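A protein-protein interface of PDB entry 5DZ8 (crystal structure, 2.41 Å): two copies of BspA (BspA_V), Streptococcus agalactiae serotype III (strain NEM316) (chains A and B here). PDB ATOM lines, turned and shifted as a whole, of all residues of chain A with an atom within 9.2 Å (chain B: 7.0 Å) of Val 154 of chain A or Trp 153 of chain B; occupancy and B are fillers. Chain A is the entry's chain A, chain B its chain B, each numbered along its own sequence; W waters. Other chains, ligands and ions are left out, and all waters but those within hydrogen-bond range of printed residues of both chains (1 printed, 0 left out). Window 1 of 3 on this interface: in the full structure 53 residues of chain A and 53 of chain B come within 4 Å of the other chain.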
ATOM      1  N   ASN A  89      11.715 -15.521   2.601  1.00  0.00           N
ATOM      2  CA  ASN A  89      12.722 -15.622   1.543  1.00  0.00           C
ATOM      3  C   ASN A  89      13.915 -14.716   1.892  1.00  0.00           C
ATOM      4  O   ASN A  89      13.749 -13.487   1.937  1.00  0.00           O
ATOM      5  CB  ASN A  89      12.084 -15.200   0.210  1.00  0.00           C
ATOM      6  CG  ASN A  89      13.010 -15.334  -0.987  1.00  0.00           C
ATOM      7  OD1 ASN A  89      14.071 -15.960  -0.929  1.00  0.00           O
ATOM      8  ND2 ASN A  89      12.591 -14.742  -2.097  1.00  0.00           N
ATOM      9  N   ALA A  91      16.659 -14.713  -0.055  1.00  0.00           N
ATOM     10  CA  ALA A  91      17.112 -14.151  -1.341  1.00  0.00           C
ATOM     11  C   ALA A  91      16.124 -13.042  -1.740  1.00  0.00           C
ATOM     12  O   ALA A  91      15.452 -13.157  -2.764  1.00  0.00           O
ATOM     13  N   VAL A  92      16.089 -11.957  -0.952  1.00  0.00           N
ATOM     14  CA  VAL A  92      14.898 -11.053  -0.819  1.00  0.00           C
ATOM     15  C   VAL A  92      14.610 -10.210  -2.085  1.00  0.00           C
ATOM     16  O   VAL A  92      13.469  -9.737  -2.278  1.00  0.00           O
ATOM     17  CB  VAL A  92      14.984 -10.128   0.461  1.00  0.00           C
ATOM     18  CG1 VAL A  92      13.621  -9.502   0.812  1.00  0.00           C
ATOM     19  CG2 VAL A  92      15.563 -10.874   1.684  1.00  0.00           C
ATOM     20  N   ASN A  93      15.634 -10.049  -2.938  1.00  0.00           N
ATOM     21  CA  ASN A  93      15.500  -9.414  -4.261  1.00  0.00           C
ATOM     22  C   ASN A  93      15.159 -10.372  -5.444  1.00  0.00           C
ATOM     23  O   ASN A  93      15.042  -9.937  -6.603  1.00  0.00           O
ATOM     24  CB  ASN A  93      16.803  -8.677  -4.565  1.00  0.00           C
ATOM     25  CG  ASN A  93      16.735  -7.853  -5.842  1.00  0.00           C
ATOM     26  OD1 ASN A  93      15.664  -7.376  -6.256  1.00  0.00           O
ATOM     27  ND2 ASN A  93      17.885  -7.694  -6.484  1.00  0.00           N
ATOM     28  N   GLN A  94      15.035 -11.668  -5.163  1.00  0.00           N
ATOM     29  CA  GLN A  94      14.700 -12.643  -6.183  1.00  0.00           C
ATOM     30  C   GLN A  94      13.201 -12.979  -6.106  1.00  0.00           C
ATOM     31  O   GLN A  94      12.578 -12.914  -5.044  1.00  0.00           O
ATOM     32  CB  GLN A  94      15.584 -13.898  -6.095  1.00  0.00           C
ATOM     33  CG  GLN A  94      17.019 -13.766  -6.657  1.00  0.00           C
ATOM     34  CD  GLN A  94      17.510 -15.037  -7.397  1.00  0.00           C
ATOM     35  OE1 GLN A  94      17.765 -15.039  -8.618  1.00  0.00           O
ATOM     36  NE2 GLN A  94      17.608 -16.131  -6.657  1.00  0.00           N
ATOM     37  N   ASN A  95      12.633 -13.287  -7.266  1.00  0.00           N
ATOM     38  CA  ASN A  95      11.253 -13.660  -7.400  1.00  0.00           C
ATOM     39  C   ASN A  95      11.147 -14.977  -8.096  1.00  0.00           C
ATOM     40  O   ASN A  95      12.084 -15.405  -8.735  1.00  0.00           O
ATOM     41  CB  ASN A  95      10.480 -12.612  -8.157  1.00  0.00           C
ATOM     42  CG  ASN A  95      10.192 -11.428  -7.289  1.00  0.00           C
ATOM     43  OD1 ASN A  95       9.679 -11.567  -6.157  1.00  0.00           O
ATOM     44  ND2 ASN A  95      10.558 -10.252  -7.778  1.00  0.00           N
ATOM     45  N   ILE A  96       9.999 -15.619  -7.918  1.00  0.00           N
ATOM     46  CA  ILE A  96       9.739 -16.928  -8.459  1.00  0.00           C
ATOM     47  C   ILE A  96       8.724 -16.784  -9.560  1.00  0.00           C
ATOM     48  O   ILE A  96       7.805 -15.993  -9.464  1.00  0.00           O
ATOM     49  CB  ILE A  96       9.212 -17.843  -7.362  1.00  0.00           C
ATOM     50  CG1 ILE A  96      10.237 -17.898  -6.227  1.00  0.00           C
ATOM     51  CG2 ILE A  96       8.952 -19.244  -7.906  1.00  0.00           C
ATOM     52  CD1 ILE A  96       9.640 -18.186  -4.865  1.00  0.00           C
ATOM     53  N   VAL A  97       8.913 -17.527 -10.626  1.00  0.00           N
ATOM     54  CA  VAL A  97       7.909 -17.632 -11.664  1.00  0.00           C
ATOM     55  C   VAL A  97       7.619 -19.109 -11.920  1.00  0.00           C
ATOM     56  O   VAL A  97       8.517 -19.867 -12.202  1.00  0.00           O
ATOM     57  CB  VAL A  97       8.351 -16.955 -12.971  1.00  0.00           C
ATOM     58  CG1 VAL A  97       7.195 -16.978 -13.977  1.00  0.00           C
ATOM     59  CG2 VAL A  97       8.770 -15.516 -12.702  1.00  0.00           C
ATOM     60  N   PHE A  98       6.357 -19.486 -11.837  1.00  0.00           N
ATOM     61  CA  PHE A  98       5.924 -20.815 -12.141  1.00  0.00           C
ATOM     62  C   PHE A  98       5.077 -20.747 -13.392  1.00  0.00           C
ATOM     63  O   PHE A  98       4.166 -19.900 -13.482  1.00  0.00           O
ATOM     64  CB  PHE A  98       5.126 -21.413 -10.972  1.00  0.00           C
ATOM     65  CG  PHE A  98       4.781 -22.867 -11.179  1.00  0.00           C
ATOM     66  CD1 PHE A  98       5.682 -23.866 -10.836  1.00  0.00           C
ATOM     67  CD2 PHE A  98       3.597 -23.223 -11.756  1.00  0.00           C
ATOM     68  CE1 PHE A  98       5.381 -25.204 -11.042  1.00  0.00           C
ATOM     69  CE2 PHE A  98       3.287 -24.546 -11.981  1.00  0.00           C
ATOM     70  CZ  PHE A  98       4.187 -25.549 -11.633  1.00  0.00           C
ATOM     71  N   ARG A  99       5.384 -21.620 -14.360  1.00  0.00           N
ATOM     72  CA  ARG A  99       4.615 -21.696 -15.590  1.00  0.00           C
ATOM     73  C   ARG A  99       4.299 -23.131 -15.955  1.00  0.00           C
ATOM     74  O   ARG A  99       5.088 -24.016 -15.747  1.00  0.00           O
ATOM     75  CB  ARG A  99       5.308 -21.115 -16.811  1.00  0.00           C
ATOM     76  CG  ARG A  99       5.752 -19.678 -16.750  1.00  0.00           C
ATOM     77  CD  ARG A  99       6.137 -19.188 -18.165  1.00  0.00           C
ATOM     78  NE  ARG A  99       6.878 -17.933 -18.054  1.00  0.00           N
ATOM     79  CZ  ARG A  99       8.141 -17.820 -17.645  1.00  0.00           C
ATOM     80  NH1 ARG A  99       8.866 -18.880 -17.326  1.00  0.00           N
ATOM     81  NH2 ARG A  99       8.695 -16.626 -17.532  1.00  0.00           N
ATOM     82  N   GLU A 110       0.745 -18.880 -15.676  1.00  0.00           N
ATOM     83  CA  GLU A 110       1.931 -18.183 -15.219  1.00  0.00           C
ATOM     84  C   GLU A 110       1.639 -17.498 -13.911  1.00  0.00           C
ATOM     85  O   GLU A 110       0.645 -16.842 -13.767  1.00  0.00           O
ATOM     86  CB  GLU A 110       2.374 -17.152 -16.236  1.00  0.00           C
ATOM     87  CG  GLU A 110       3.693 -16.525 -15.829  1.00  0.00           C
ATOM     88  CD  GLU A 110       4.369 -15.733 -16.949  1.00  0.00           C
ATOM     89  OE1 GLU A 110       4.368 -16.128 -18.155  1.00  0.00           O
ATOM     90  OE2 GLU A 110       4.912 -14.696 -16.587  1.00  0.00           O
ATOM     91  N   LYS A 111       2.539 -17.634 -12.962  1.00  0.00           N
ATOM     92  CA  LYS A 111       2.386 -17.001 -11.685  1.00  0.00           C
ATOM     93  C   LYS A 111       3.743 -16.579 -11.168  1.00  0.00           C
ATOM     94  O   LYS A 111       4.633 -17.417 -10.911  1.00  0.00           O
ATOM     95  CB  LYS A 111       1.771 -17.994 -10.731  1.00  0.00           C
ATOM     96  CG  LYS A 111       1.602 -17.489  -9.317  1.00  0.00           C
ATOM     97  CD  LYS A 111       0.464 -16.481  -9.179  1.00  0.00           C
ATOM     98  CE  LYS A 111       0.433 -16.050  -7.714  1.00  0.00           C
ATOM     99  NZ  LYS A 111      -0.791 -15.307  -7.437  1.00  0.00           N
ATOM    100  N   ALA A 112       3.875 -15.270 -11.001  1.00  0.00           N
ATOM    101  CA  ALA A 112       5.075 -14.660 -10.511  1.00  0.00           C
ATOM    102  C   ALA A 112       4.782 -14.272  -9.060  1.00  0.00           C
ATOM    103  O   ALA A 112       3.715 -13.750  -8.775  1.00  0.00           O
ATOM    104  CB  ALA A 112       5.378 -13.445 -11.348  1.00  0.00           C
ATOM    105  N   HIS A 113       5.698 -14.562  -8.148  1.00  0.00           N
ATOM    106  CA  HIS A 113       5.468 -14.287  -6.732  1.00  0.00           C
ATOM    107  C   HIS A 113       6.815 -14.305  -6.007  1.00  0.00           C
ATOM    108  O   HIS A 113       7.816 -14.791  -6.574  1.00  0.00           O
ATOM    109  CB  HIS A 113       4.458 -15.307  -6.114  1.00  0.00           C
ATOM    110  CG  HIS A 113       4.959 -16.720  -6.078  1.00  0.00           C
ATOM    111  ND1 HIS A 113       5.378 -17.343  -4.922  1.00  0.00           N
ATOM    112  CD2 HIS A 113       5.125 -17.627  -7.064  1.00  0.00           C
ATOM    113  CE1 HIS A 113       5.745 -18.576  -5.185  1.00  0.00           C
ATOM    114  NE2 HIS A 113       5.620 -18.772  -6.482  1.00  0.00           N
ATOM    115  N   ASN A 114       6.827 -13.785  -4.776  1.00  0.00           N
ATOM    116  CA  ASN A 114       8.037 -13.634  -3.959  1.00  0.00           C
ATOM    117  C   ASN A 114       8.271 -14.785  -2.965  1.00  0.00           C
ATOM    118  O   ASN A 114       9.250 -14.781  -2.205  1.00  0.00           O
ATOM    119  CB  ASN A 114       7.999 -12.330  -3.186  1.00  0.00           C
ATOM    120  CG  ASN A 114       6.882 -12.293  -2.141  1.00  0.00           C
ATOM    121  OD1 ASN A 114       6.402 -13.331  -1.634  1.00  0.00           O
ATOM    122  ND2 ASN A 114       6.428 -11.095  -1.849  1.00  0.00           N
ATOM    123  N   ASP A 151       9.950 -23.468 -13.384  1.00  0.00           N
ATOM    124  CA  ASP A 151       9.957 -23.035 -12.016  1.00  0.00           C
ATOM    125  C   ASP A 151      11.263 -22.302 -11.801  1.00  0.00           C
ATOM    126  O   ASP A 151      12.283 -22.922 -11.485  1.00  0.00           O
ATOM    127  CB  ASP A 151       9.821 -24.241 -11.108  1.00  0.00           C
ATOM    128  CG  ASP A 151       9.734 -23.863  -9.655  1.00  0.00           C
ATOM    129  OD1 ASP A 151       9.009 -22.861  -9.303  1.00  0.00           O
ATOM    130  OD2 ASP A 151      10.384 -24.603  -8.878  1.00  0.00           O
ATOM    131  N   ASP A 152      11.202 -20.984 -11.992  1.00  0.00           N
ATOM    132  CA  ASP A 152      12.370 -20.153 -12.191  1.00  0.00           C
ATOM    133  C   ASP A 152      12.552 -19.156 -11.046  1.00  0.00           C
ATOM    134  O   ASP A 152      11.569 -18.672 -10.462  1.00  0.00           O
ATOM    135  CB  ASP A 152      12.207 -19.449 -13.547  1.00  0.00           C
ATOM    136  CG  ASP A 152      12.254 -20.446 -14.715  1.00  0.00           C
ATOM    137  OD1 ASP A 152      12.553 -21.643 -14.451  1.00  0.00           O
ATOM    138  OD2 ASP A 152      11.992 -20.077 -15.890  1.00  0.00           O
ATOM    139  N   TRP A 153      13.812 -18.893 -10.719  1.00  0.00           N
ATOM    140  CA  TRP A 153      14.223 -17.764  -9.855  1.00  0.00           C
ATOM    141  C   TRP A 153      14.634 -16.564 -10.731  1.00  0.00           C
ATOM    142  O   TRP A 153      15.489 -16.704 -11.597  1.00  0.00           O
ATOM    143  CB  TRP A 153      15.403 -18.156  -8.932  1.00  0.00           C
ATOM    144  CG  TRP A 153      15.003 -18.861  -7.670  1.00  0.00           C
ATOM    145  CD1 TRP A 153      15.159 -20.196  -7.383  1.00  0.00           C
ATOM    146  CD2 TRP A 153      14.348 -18.281  -6.518  1.00  0.00           C
ATOM    147  NE1 TRP A 153      14.645 -20.470  -6.129  1.00  0.00           N
ATOM    148  CE2 TRP A 153      14.151 -19.312  -5.582  1.00  0.00           C
ATOM    149  CE3 TRP A 153      13.908 -16.997  -6.202  1.00  0.00           C
ATOM    150  CZ2 TRP A 153      13.563 -19.091  -4.348  1.00  0.00           C
ATOM    151  CZ3 TRP A 153      13.310 -16.776  -4.974  1.00  0.00           C
ATOM    152  CH2 TRP A 153      13.143 -17.820  -4.064  1.00  0.00           C
ATOM    153  N   VAL A 154      14.023 -15.407 -10.516  1.00  0.00           N
ATOM    154  CA  VAL A 154      14.313 -14.191 -11.285  1.00  0.00           C
ATOM    155  C   VAL A 154      14.927 -13.128 -10.391  1.00  0.00           C
ATOM    156  O   VAL A 154      14.371 -12.795  -9.370  1.00  0.00           O
ATOM    157  CB  VAL A 154      13.035 -13.639 -11.916  1.00  0.00           C
ATOM    158  CG1 VAL A 154      13.321 -12.363 -12.700  1.00  0.00           C
ATOM    159  CG2 VAL A 154      12.437 -14.713 -12.820  1.00  0.00           C
ATOM    160  N   HIS A 155      16.078 -12.607 -10.786  1.00  0.00           N
ATOM    161  CA  HIS A 155      16.763 -11.495 -10.101  1.00  0.00           C
ATOM    162  C   HIS A 155      16.874 -10.306 -11.079  1.00  0.00           C
ATOM    163  O   HIS A 155      17.701 -10.323 -11.996  1.00  0.00           O
ATOM    164  CB  HIS A 155      18.148 -11.941  -9.692  1.00  0.00           C
ATOM    165  CG  HIS A 155      18.916 -10.930  -8.907  1.00  0.00           C
ATOM    166  ND1 HIS A 155      19.431 -11.207  -7.659  1.00  0.00           N
ATOM    167  CD2 HIS A 155      19.296  -9.666  -9.199  1.00  0.00           C
ATOM    168  CE1 HIS A 155      20.087 -10.154  -7.210  1.00  0.00           C
ATOM    169  NE2 HIS A 155      20.013  -9.205  -8.123  1.00  0.00           N
ATOM    170  N   ASP A 156      16.051  -9.289 -10.838  1.00  0.00           N
ATOM    171  CA  ASP A 156      15.862  -8.159 -11.718  1.00  0.00           C
ATOM    172  C   ASP A 156      16.445  -6.913 -11.063  1.00  0.00           C
ATOM    173  O   ASP A 156      15.785  -6.339 -10.189  1.00  0.00           O
ATOM    174  CB  ASP A 156      14.381  -7.931 -11.959  1.00  0.00           C
ATOM    175  CG  ASP A 156      13.781  -8.872 -13.023  1.00  0.00           C
ATOM    176  OD1 ASP A 156      14.512  -9.558 -13.779  1.00  0.00           O
ATOM    177  OD2 ASP A 156      12.531  -8.934 -13.107  1.00  0.00           O
ATOM    178  N   THR A 157      17.672  -6.523 -11.455  1.00  0.00           N
ATOM    179  CA  THR A 157      18.237  -5.201 -11.105  1.00  0.00           C
ATOM    180  C   THR A 157      17.817  -4.141 -12.164  1.00  0.00           C
ATOM    181  O   THR A 157      18.495  -3.949 -13.171  1.00  0.00           O
ATOM    182  CB  THR A 157      19.771  -5.257 -10.971  1.00  0.00           C
ATOM    183  OG1 THR A 157      20.158  -6.291 -10.056  1.00  0.00           O
ATOM    184  CG2 THR A 157      20.332  -3.922 -10.457  1.00  0.00           C
ATOM    185  N   HIS A 158      16.671  -3.491 -11.952  1.00  0.00           N
ATOM    186  CA  HIS A 158      16.138  -2.462 -12.850  1.00  0.00           C
ATOM    187  C   HIS A 158      16.512  -1.056 -12.369  1.00  0.00           C
ATOM    188  O   HIS A 158      16.137  -0.649 -11.272  1.00  0.00           O
ATOM    189  CB  HIS A 158      14.639  -2.629 -12.988  1.00  0.00           C
ATOM    190  CG  HIS A 158      14.279  -3.795 -13.840  1.00  0.00           C
ATOM    191  ND1 HIS A 158      13.215  -3.780 -14.713  1.00  0.00           N
ATOM    192  CD2 HIS A 158      14.909  -4.983 -14.026  1.00  0.00           C
ATOM    193  CE1 HIS A 158      13.186  -4.921 -15.378  1.00  0.00           C
ATOM    194  NE2 HIS A 158      14.208  -5.665 -14.983  1.00  0.00           N
ATOM    195  N   MET B  41      28.422  -9.305 -12.264  1.00  0.00           N
ATOM    196  CA  MET B  41      27.471 -10.441 -12.126  1.00  0.00           C
ATOM    197  C   MET B  41      28.028 -11.325 -11.030  1.00  0.00           C
ATOM    198  O   MET B  41      29.236 -11.595 -11.019  1.00  0.00           O
ATOM    199  CB  MET B  41      27.307 -11.223 -13.433  1.00  0.00           C
ATOM    200  CG  MET B  41      26.530 -10.488 -14.539  1.00  0.00           C
ATOM    201  SD  MET B  41      24.603 -10.104 -14.219  1.00  0.00           S
ATOM    202  CE  MET B  41      23.945 -11.688 -13.234  1.00  0.00           C
ATOM    203  N   ILE B  42      27.165 -11.798 -10.118  1.00  0.00           N
ATOM    204  CA  ILE B  42      27.604 -12.266  -8.782  1.00  0.00           C
ATOM    205  C   ILE B  42      27.564 -13.785  -8.484  1.00  0.00           C
ATOM    206  O   ILE B  42      28.444 -14.284  -7.759  1.00  0.00           O
ATOM    207  CB  ILE B  42      26.881 -11.450  -7.674  1.00  0.00           C
ATOM    208  CG1 ILE B  42      27.798 -11.299  -6.443  1.00  0.00           C
ATOM    209  CG2 ILE B  42      25.473 -11.999  -7.375  1.00  0.00           C
ATOM    210  CD1 ILE B  42      28.958 -10.328  -6.656  1.00  0.00           C
ATOM    211  N   ASP B  43      26.565 -14.496  -9.025  1.00  0.00           N
ATOM    212  CA  ASP B  43      26.438 -15.981  -8.928  1.00  0.00           C
ATOM    213  C   ASP B  43      26.095 -16.476  -7.521  1.00  0.00           C
ATOM    214  O   ASP B  43      24.910 -16.653  -7.202  1.00  0.00           O
ATOM    215  CB  ASP B  43      27.690 -16.691  -9.459  1.00  0.00           C
ATOM    216  N   GLY B  44      27.127 -16.730  -6.707  1.00  0.00           N
ATOM    217  CA  GLY B  44      26.972 -16.905  -5.267  1.00  0.00           C
ATOM    218  C   GLY B  44      27.527 -15.659  -4.603  1.00  0.00           C
ATOM    219  O   GLY B  44      26.916 -14.586  -4.656  1.00  0.00           O
ATOM    220  N   GLN B  94      21.556 -20.746 -16.829  1.00  0.00           N
ATOM    221  CA  GLN B  94      21.579 -19.327 -16.547  1.00  0.00           C
ATOM    222  C   GLN B  94      21.283 -18.558 -17.826  1.00  0.00           C
ATOM    223  O   GLN B  94      21.955 -18.704 -18.856  1.00  0.00           O
ATOM    224  CB  GLN B  94      22.938 -18.950 -15.965  1.00  0.00           C
ATOM    225  CG  GLN B  94      23.122 -19.382 -14.514  1.00  0.00           C
ATOM    226  CD  GLN B  94      22.180 -18.641 -13.588  1.00  0.00           C
ATOM    227  OE1 GLN B  94      21.789 -17.514 -13.886  1.00  0.00           O
ATOM    228  NE2 GLN B  94      21.793 -19.269 -12.472  1.00  0.00           N
ATOM    229  N   ASN B  95      20.200 -17.809 -17.773  1.00  0.00           N
ATOM    230  CA  ASN B  95      19.915 -16.810 -18.749  1.00  0.00           C
ATOM    231  C   ASN B  95      20.212 -15.475 -18.036  1.00  0.00           C
ATOM    232  O   ASN B  95      19.781 -15.245 -16.901  1.00  0.00           O
ATOM    233  CB  ASN B  95      18.455 -16.952 -19.216  1.00  0.00           C
ATOM    234  CG  ASN B  95      18.186 -16.319 -20.589  1.00  0.00           C
ATOM    235  OD1 ASN B  95      19.067 -16.237 -21.456  1.00  0.00           O
ATOM    236  ND2 ASN B  95      16.940 -15.878 -20.794  1.00  0.00           N
ATOM    237  N   ILE B  96      21.049 -14.654 -18.668  1.00  0.00           N
ATOM    238  CA  ILE B  96      21.351 -13.295 -18.219  1.00  0.00           C
ATOM    239  C   ILE B  96      20.927 -12.409 -19.340  1.00  0.00           C
ATOM    240  O   ILE B  96      21.130 -12.749 -20.486  1.00  0.00           O
ATOM    241  CB  ILE B  96      22.826 -13.087 -17.975  1.00  0.00           C
ATOM    242  CG1 ILE B  96      23.244 -13.830 -16.713  1.00  0.00           C
ATOM    243  CG2 ILE B  96      23.150 -11.606 -17.860  1.00  0.00           C
ATOM    244  CD1 ILE B  96      24.745 -13.877 -16.488  1.00  0.00           C
ATOM    245  N   VAL B  97      20.296 -11.287 -19.025  1.00  0.00           N
ATOM    246  CA  VAL B  97      19.910 -10.373 -20.080  1.00  0.00           C
ATOM    247  C   VAL B  97      20.273  -8.951 -19.632  1.00  0.00           C
ATOM    248  O   VAL B  97      20.038  -8.524 -18.470  1.00  0.00           O
ATOM    249  CB  VAL B  97      18.456 -10.613 -20.518  1.00  0.00           C
ATOM    250  CG1 VAL B  97      17.504 -10.530 -19.346  1.00  0.00           C
ATOM    251  CG2 VAL B  97      18.034  -9.665 -21.626  1.00  0.00           C
ATOM    252  N   ASP B 151      19.461  -5.372 -15.755  1.00  0.00           N
ATOM    253  CA  ASP B 151      20.512  -6.374 -15.684  1.00  0.00           C
ATOM    254  C   ASP B 151      20.014  -7.618 -14.975  1.00  0.00           C
ATOM    255  O   ASP B 151      20.458  -7.956 -13.866  1.00  0.00           O
ATOM    256  CB  ASP B 151      21.753  -5.817 -15.020  1.00  0.00           C
ATOM    257  CG  ASP B 151      22.913  -6.798 -15.049  1.00  0.00           C
ATOM    258  OD1 ASP B 151      23.075  -7.543 -16.074  1.00  0.00           O
ATOM    259  OD2 ASP B 151      23.653  -6.806 -14.029  1.00  0.00           O
ATOM    260  N   ASP B 152      19.123  -8.306 -15.689  1.00  0.00           N
ATOM    261  CA  ASP B 152      18.350  -9.441 -15.183  1.00  0.00           C
ATOM    262  C   ASP B 152      19.043 -10.788 -15.325  1.00  0.00           C
ATOM    263  O   ASP B 152      19.896 -11.026 -16.189  1.00  0.00           O
ATOM    264  CB  ASP B 152      16.976  -9.471 -15.864  1.00  0.00           C
ATOM    265  CG  ASP B 152      16.258  -8.148 -15.712  1.00  0.00           C
ATOM    266  OD1 ASP B 152      16.776  -7.346 -14.893  1.00  0.00           O
ATOM    267  OD2 ASP B 152      15.236  -7.892 -16.395  1.00  0.00           O
ATOM    268  N   TRP B 153      18.618 -11.684 -14.463  1.00  0.00           N
ATOM    269  CA  TRP B 153      19.357 -12.870 -14.171  1.00  0.00           C
ATOM    270  C   TRP B 153      18.274 -13.880 -13.809  1.00  0.00           C
ATOM    271  O   TRP B 153      17.537 -13.673 -12.860  1.00  0.00           O
ATOM    272  CB  TRP B 153      20.307 -12.492 -13.050  1.00  0.00           C
ATOM    273  CG  TRP B 153      21.152 -13.545 -12.556  1.00  0.00           C
ATOM    274  CD1 TRP B 153      21.758 -14.527 -13.282  1.00  0.00           C
ATOM    275  CD2 TRP B 153      21.562 -13.725 -11.200  1.00  0.00           C
ATOM    276  NE1 TRP B 153      22.503 -15.336 -12.449  1.00  0.00           N
ATOM    277  CE2 TRP B 153      22.396 -14.864 -11.163  1.00  0.00           C
ATOM    278  CE3 TRP B 153      21.295 -13.042 -10.003  1.00  0.00           C
ATOM    279  CZ2 TRP B 153      22.963 -15.342  -9.959  1.00  0.00           C
ATOM    280  CZ3 TRP B 153      21.851 -13.515  -8.806  1.00  0.00           C
ATOM    281  CH2 TRP B 153      22.676 -14.654  -8.797  1.00  0.00           C
ATOM    282  N   VAL B 154      18.116 -14.900 -14.651  1.00  0.00           N
ATOM    283  CA  VAL B 154      17.190 -15.998 -14.400  1.00  0.00           C
ATOM    284  C   VAL B 154      17.935 -17.297 -14.158  1.00  0.00           C
ATOM    285  O   VAL B 154      18.780 -17.686 -14.960  1.00  0.00           O
ATOM    286  CB  VAL B 154      16.249 -16.251 -15.585  1.00  0.00           C
ATOM    287  CG1 VAL B 154      15.287 -17.397 -15.254  1.00  0.00           C
ATOM    288  CG2 VAL B 154      15.465 -14.991 -15.928  1.00  0.00           C
ATOM    289  N   HIS B 155      17.599 -17.983 -13.073  1.00  0.00           N
ATOM    290  CA  HIS B 155      18.009 -19.378 -12.891  1.00  0.00           C
ATOM    291  C   HIS B 155      16.862 -20.318 -13.307  1.00  0.00           C
ATOM    292  O   HIS B 155      15.884 -20.447 -12.585  1.00  0.00           O
ATOM    293  CB  HIS B 155      18.467 -19.650 -11.453  1.00  0.00           C
ATOM    294  CG  HIS B 155      18.739 -21.102 -11.206  1.00  0.00           C
ATOM    295  ND1 HIS B 155      18.077 -21.838 -10.243  1.00  0.00           N
ATOM    296  CD2 HIS B 155      19.526 -21.981 -11.874  1.00  0.00           C
ATOM    297  CE1 HIS B 155      18.488 -23.093 -10.292  1.00  0.00           C
ATOM    298  NE2 HIS B 155      19.362 -23.206 -11.277  1.00  0.00           N
HETATM  299  O   HOH W   1      15.015 -22.668 -10.651  1.00  0.00           O
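Hydrophobic or aromatic side chains of chain B that line the printed part of chain A: Trp 153 and Val 154.
Of the 23 printed residues of chain A, 7 touch a printed residue of chain B.
Hydrophobic or aromatic side chains of chain A within 4 Å of the printed part of chain B: His 155 and His 158.
Asn 89 of chain A touches none of the printed residues of chain B.
Ile 96 of chain A touches none of the printed residues of chain B.
Of chain B, only Trp 153 comes within 4 Å of Val 154 of chain A.
Of the printed residues of chain B, His 155 of chain A touches Asp 152 and Trp 153.
Printed residues of chain B within 4 Å of His 158 of chain A: Asp 152.
Asp 43 of chain B touches none of the printed residues of chain A.
Trp 153 of chain B touches three residues of chain A.
Val 154 of chain B touches just one residue of chain A: Trp 153.
The nearest residue of chain A that does not touch Trp 153 of chain B is Gln 94 of chain A (4.3 Å).
The nearest printed residue of chain B that does not touch Trp 153 of chain A is Gln 94 of chain B (6.8 Å).
Asp 152 of chain A touches His 155 of chain B, and with the chains exchanged His 155 of chain A touches Asp 152 of chain B.
Trp 153 of chain A touches its own counterpart, Trp 153 of chain B.
Trp 153 of chain A touches Val 154 of chain B, and with the chains exchanged Val 154 of chain A touches Trp 153 of chain B.
Trp 153 of chain A touches His 155 of chain B, and with the chains exchanged His 155 of chain A touches Trp 153 of chain B.
Positions printed for both chains: 94, 95, 96, 97, 151, 152, 153, 154 and 155.
Of the 11 pairs that touch across the chains among the printed residues, 7 have their exchanged pair printed and touching as well.
Water W1 lies within hydrogen-bond range of O of Asp 151 of chain A (2.9 Å) and O of His 155 of chain B (3.1 Å).
The side-chain amide nitrogen (ND2) of Asn 93 of chain A is in hydrogen-bond range of a ring nitrogen (NE2) of His 155 of chain A (3.1 Å).
The side-chain amide oxygen (OE1) of Gln 94 of chain B lies close to the backbone carbonyl oxygen (O) of Val 154 of chain B (3.2 Å).
The backbone NH (N) of Val 154 of chain B is in hydrogen-bond range of the backbone carbonyl oxygen (O) of Asn 95 of chain B (2.8 Å).
The side-chain amide oxygen (OE1) of Gln 94 of chain B lies within hydrogen-bond range of the indole nitrogen (NE1) of Trp 153 of chain B, 2.7 Å away.
A ring nitrogen (NE2) of His 155 of chain A sits at hydrogen-bond distance from the side-chain hydroxyl of Thr 157 of chain A (3.5 Å).
The backbone NH (N) of Val 97 of chain B sits at hydrogen-bond distance from the backbone carbonyl oxygen (O) of Asp 152 of chain B.
The side-chain carboxylate (OD1) of Asp 156 of chain A sits close to the side-chain carboxylate (OD2) of Asp 152 of chain B (3.2 Å).
The side-chain carboxylate (OD2) of Asp 152 of chain B lies within hydrogen-bond range of a ring nitrogen (NE2) of His 158 of chain A, at 2.8 Å.
The backbone carbonyl oxygen (O) of Trp 153 of chain A is in hydrogen-bond range of the backbone NH (N) of His 155 of chain B (2.9 Å).
The backbone NH of His 155 of chain A sits at hydrogen-bond distance from the backbone carbonyl oxygen of Trp 153 of chain B (2.8 Å).
The backbone NH (N) of Asp 151 of chain B lies within hydrogen-bond range of the backbone carbonyl oxygen (O) of Thr 157 of chain A (3.1 Å).
Among the printed residues, merely in contact across the chains: Trp 153 of chain A with Val 154 of chain B (3.4 Å), His 155 of chain A with Asp 152 of chain B (3.4 Å), Asp 152 of chain A with His 155 of chain B (3.5 Å), Val 154 of chain A with Trp 153 of chain B (3.6 Å), Thr 157 of chain A with Asp 152 of chain B (3.6 Å) and Trp 153 of chain A with Trp 153 of chain B (3.9 Å).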
